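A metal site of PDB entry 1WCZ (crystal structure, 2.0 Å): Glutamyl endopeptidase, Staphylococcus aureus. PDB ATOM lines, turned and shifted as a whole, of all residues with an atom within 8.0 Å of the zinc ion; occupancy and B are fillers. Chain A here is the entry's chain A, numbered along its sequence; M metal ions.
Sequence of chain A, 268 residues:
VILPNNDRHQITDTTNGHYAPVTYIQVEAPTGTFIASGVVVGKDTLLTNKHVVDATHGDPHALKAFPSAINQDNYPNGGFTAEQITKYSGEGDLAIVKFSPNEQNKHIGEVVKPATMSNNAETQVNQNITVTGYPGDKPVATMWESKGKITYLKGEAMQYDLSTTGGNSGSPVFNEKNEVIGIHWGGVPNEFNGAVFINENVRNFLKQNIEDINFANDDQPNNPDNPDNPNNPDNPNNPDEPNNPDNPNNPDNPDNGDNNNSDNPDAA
The nearest printed residue that does not touch the zinc ion is Arg 8 (5.1 Å).
ND2 of Asn 5 sits at hydrogen-bond distance from O of Lys 147, 3.0 Å away.
O of His 9 lies within hydrogen-bond range of N of Glu 145 (2.7 Å).
The zinc ion is bound by the side-chain carboxylate (OD2) of Asp 7, 2.0 Å away.
The zinc ion is bound by a ring nitrogen (NE2) of His 9, at 2.1 Å.
NZ of Lys 147 binds the zinc ion (2.1 Å).
OD1 of Asp 7 binds the zinc ion (2.6 Å).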
ATOM      1  N   ASN A   5     -19.820 -15.979  33.094  1.00  0.00           N
ATOM      2  CA  ASN A   5     -20.816 -16.126  32.041  1.00  0.00           C
ATOM      3  C   ASN A   5     -21.584 -14.814  31.940  1.00  0.00           C
ATOM      4  O   ASN A   5     -22.443 -14.519  32.786  1.00  0.00           O
ATOM      5  CB  ASN A   5     -21.784 -17.271  32.362  1.00  0.00           C
ATOM      6  CG  ASN A   5     -23.028 -17.249  31.480  1.00  0.00           C
ATOM      7  OD1 ASN A   5     -22.973 -16.840  30.312  1.00  0.00           O
ATOM      8  ND2 ASN A   5     -24.157 -17.696  32.032  1.00  0.00           N
ATOM      9  N   ASN A   6     -21.263 -14.018  30.924  1.00  0.00           N
ATOM     10  CA  ASN A   6     -21.915 -12.749  30.685  1.00  0.00           C
ATOM     11  C   ASN A   6     -22.469 -12.781  29.266  1.00  0.00           C
ATOM     12  O   ASN A   6     -21.837 -12.298  28.326  1.00  0.00           O
ATOM     13  CB  ASN A   6     -20.908 -11.603  30.813  1.00  0.00           C
ATOM     14  CG  ASN A   6     -21.562 -10.228  30.775  1.00  0.00           C
ATOM     15  OD1 ASN A   6     -20.888  -9.208  30.926  1.00  0.00           O
ATOM     16  ND2 ASN A   6     -22.873 -10.199  30.575  1.00  0.00           N
ATOM     17  N   ASP A   7     -23.647 -13.371  29.130  1.00  0.00           N
ATOM     18  CA  ASP A   7     -24.275 -13.570  27.824  1.00  0.00           C
ATOM     19  C   ASP A   7     -25.622 -12.863  27.794  1.00  0.00           C
ATOM     20  O   ASP A   7     -26.653 -13.439  28.165  1.00  0.00           O
ATOM     21  CB  ASP A   7     -24.436 -15.069  27.573  1.00  0.00           C
ATOM     22  CG  ASP A   7     -25.046 -15.365  26.225  1.00  0.00           C
ATOM     23  OD1 ASP A   7     -25.133 -16.562  25.874  1.00  0.00           O
ATOM     24  OD2 ASP A   7     -25.442 -14.416  25.526  1.00  0.00           O
ATOM     25  N   ARG A   8     -25.607 -11.618  27.348  1.00  0.00           N
ATOM     26  CA  ARG A   8     -26.801 -10.786  27.324  1.00  0.00           C
ATOM     27  C   ARG A   8     -27.100 -10.183  25.948  1.00  0.00           C
ATOM     28  O   ARG A   8     -26.185  -9.738  25.253  1.00  0.00           O
ATOM     29  CB  ARG A   8     -26.666  -9.675  28.368  1.00  0.00           C
ATOM     30  CG  ARG A   8     -26.316 -10.215  29.752  1.00  0.00           C
ATOM     31  CD  ARG A   8     -26.320  -9.107  30.795  1.00  0.00           C
ATOM     32  NE  ARG A   8     -25.088  -8.324  30.770  1.00  0.00           N
ATOM     33  CZ  ARG A   8     -24.948  -7.144  31.353  1.00  0.00           C
ATOM     34  NH1 ARG A   8     -25.958  -6.603  32.016  1.00  0.00           N
ATOM     35  NH2 ARG A   8     -23.780  -6.504  31.273  1.00  0.00           N
ATOM     36  N   HIS A   9     -28.378 -10.184  25.581  1.00  0.00           N
ATOM     37  CA  HIS A   9     -28.819  -9.655  24.286  1.00  0.00           C
ATOM     38  C   HIS A   9     -29.906  -8.606  24.513  1.00  0.00           C
ATOM     39  O   HIS A   9     -30.804  -8.807  25.325  1.00  0.00           O
ATOM     40  CB  HIS A   9     -29.426 -10.768  23.437  1.00  0.00           C
ATOM     41  CG  HIS A   9     -28.502 -11.908  23.160  1.00  0.00           C
ATOM     42  ND1 HIS A   9     -28.192 -12.314  21.875  1.00  0.00           N
ATOM     43  CD2 HIS A   9     -27.829 -12.746  23.987  1.00  0.00           C
ATOM     44  CE1 HIS A   9     -27.375 -13.356  21.933  1.00  0.00           C
ATOM     45  NE2 HIS A   9     -27.144 -13.632  23.209  1.00  0.00           N
ATOM     46  N   GLU A 145     -31.860  -9.590  27.719  1.00  0.00           N
ATOM     47  CA  GLU A 145     -32.069 -10.965  28.126  1.00  0.00           C
ATOM     48  C   GLU A 145     -30.704 -11.544  28.500  1.00  0.00           C
ATOM     49  O   GLU A 145     -29.766 -11.474  27.708  1.00  0.00           O
ATOM     50  CB  GLU A 145     -32.666 -11.753  26.965  1.00  0.00           C
ATOM     51  CG  GLU A 145     -32.850 -13.230  27.204  1.00  0.00           C
ATOM     52  CD  GLU A 145     -33.476 -13.929  26.007  1.00  0.00           C
ATOM     53  OE1 GLU A 145     -32.723 -14.357  25.099  1.00  0.00           O
ATOM     54  OE2 GLU A 145     -34.724 -14.043  25.957  1.00  0.00           O
ATOM     55  N   SER A 146     -30.591 -12.090  29.708  1.00  0.00           N
ATOM     56  CA  SER A 146     -29.327 -12.697  30.156  1.00  0.00           C
ATOM     57  C   SER A 146     -29.470 -14.218  30.235  1.00  0.00           C
ATOM     58  O   SER A 146     -30.376 -14.739  30.892  1.00  0.00           O
ATOM     59  CB  SER A 146     -28.934 -12.149  31.526  1.00  0.00           C
ATOM     60  OG  SER A 146     -27.735 -12.749  31.981  1.00  0.00           O
ATOM     61  N   LYS A 147     -28.567 -14.929  29.561  1.00  0.00           N
ATOM     62  CA  LYS A 147     -28.635 -16.389  29.474  1.00  0.00           C
ATOM     63  C   LYS A 147     -27.674 -17.115  30.397  1.00  0.00           C
ATOM     64  O   LYS A 147     -26.542 -16.668  30.625  1.00  0.00           O
ATOM     65  CB  LYS A 147     -28.361 -16.828  28.034  1.00  0.00           C
ATOM     66  CG  LYS A 147     -29.303 -16.212  26.995  1.00  0.00           C
ATOM     67  CD  LYS A 147     -28.590 -15.951  25.673  1.00  0.00           C
ATOM     68  CE  LYS A 147     -28.071 -17.243  25.054  1.00  0.00           C
ATOM     69  NZ  LYS A 147     -27.363 -16.996  23.748  1.00  0.00           N
ATOM     70  N   GLY A 148     -28.133 -18.244  30.924  1.00  0.00           N
ATOM     71  CA  GLY A 148     -27.324 -19.052  31.825  1.00  0.00           C
ATOM     72  C   GLY A 148     -28.046 -20.318  32.264  1.00  0.00           C
ATOM     73  O   GLY A 148     -29.062 -20.699  31.682  1.00  0.00           O
HETATM   74 ZN    ZN M   1     -26.095 -15.313  23.813  1.00  0.00          ZN
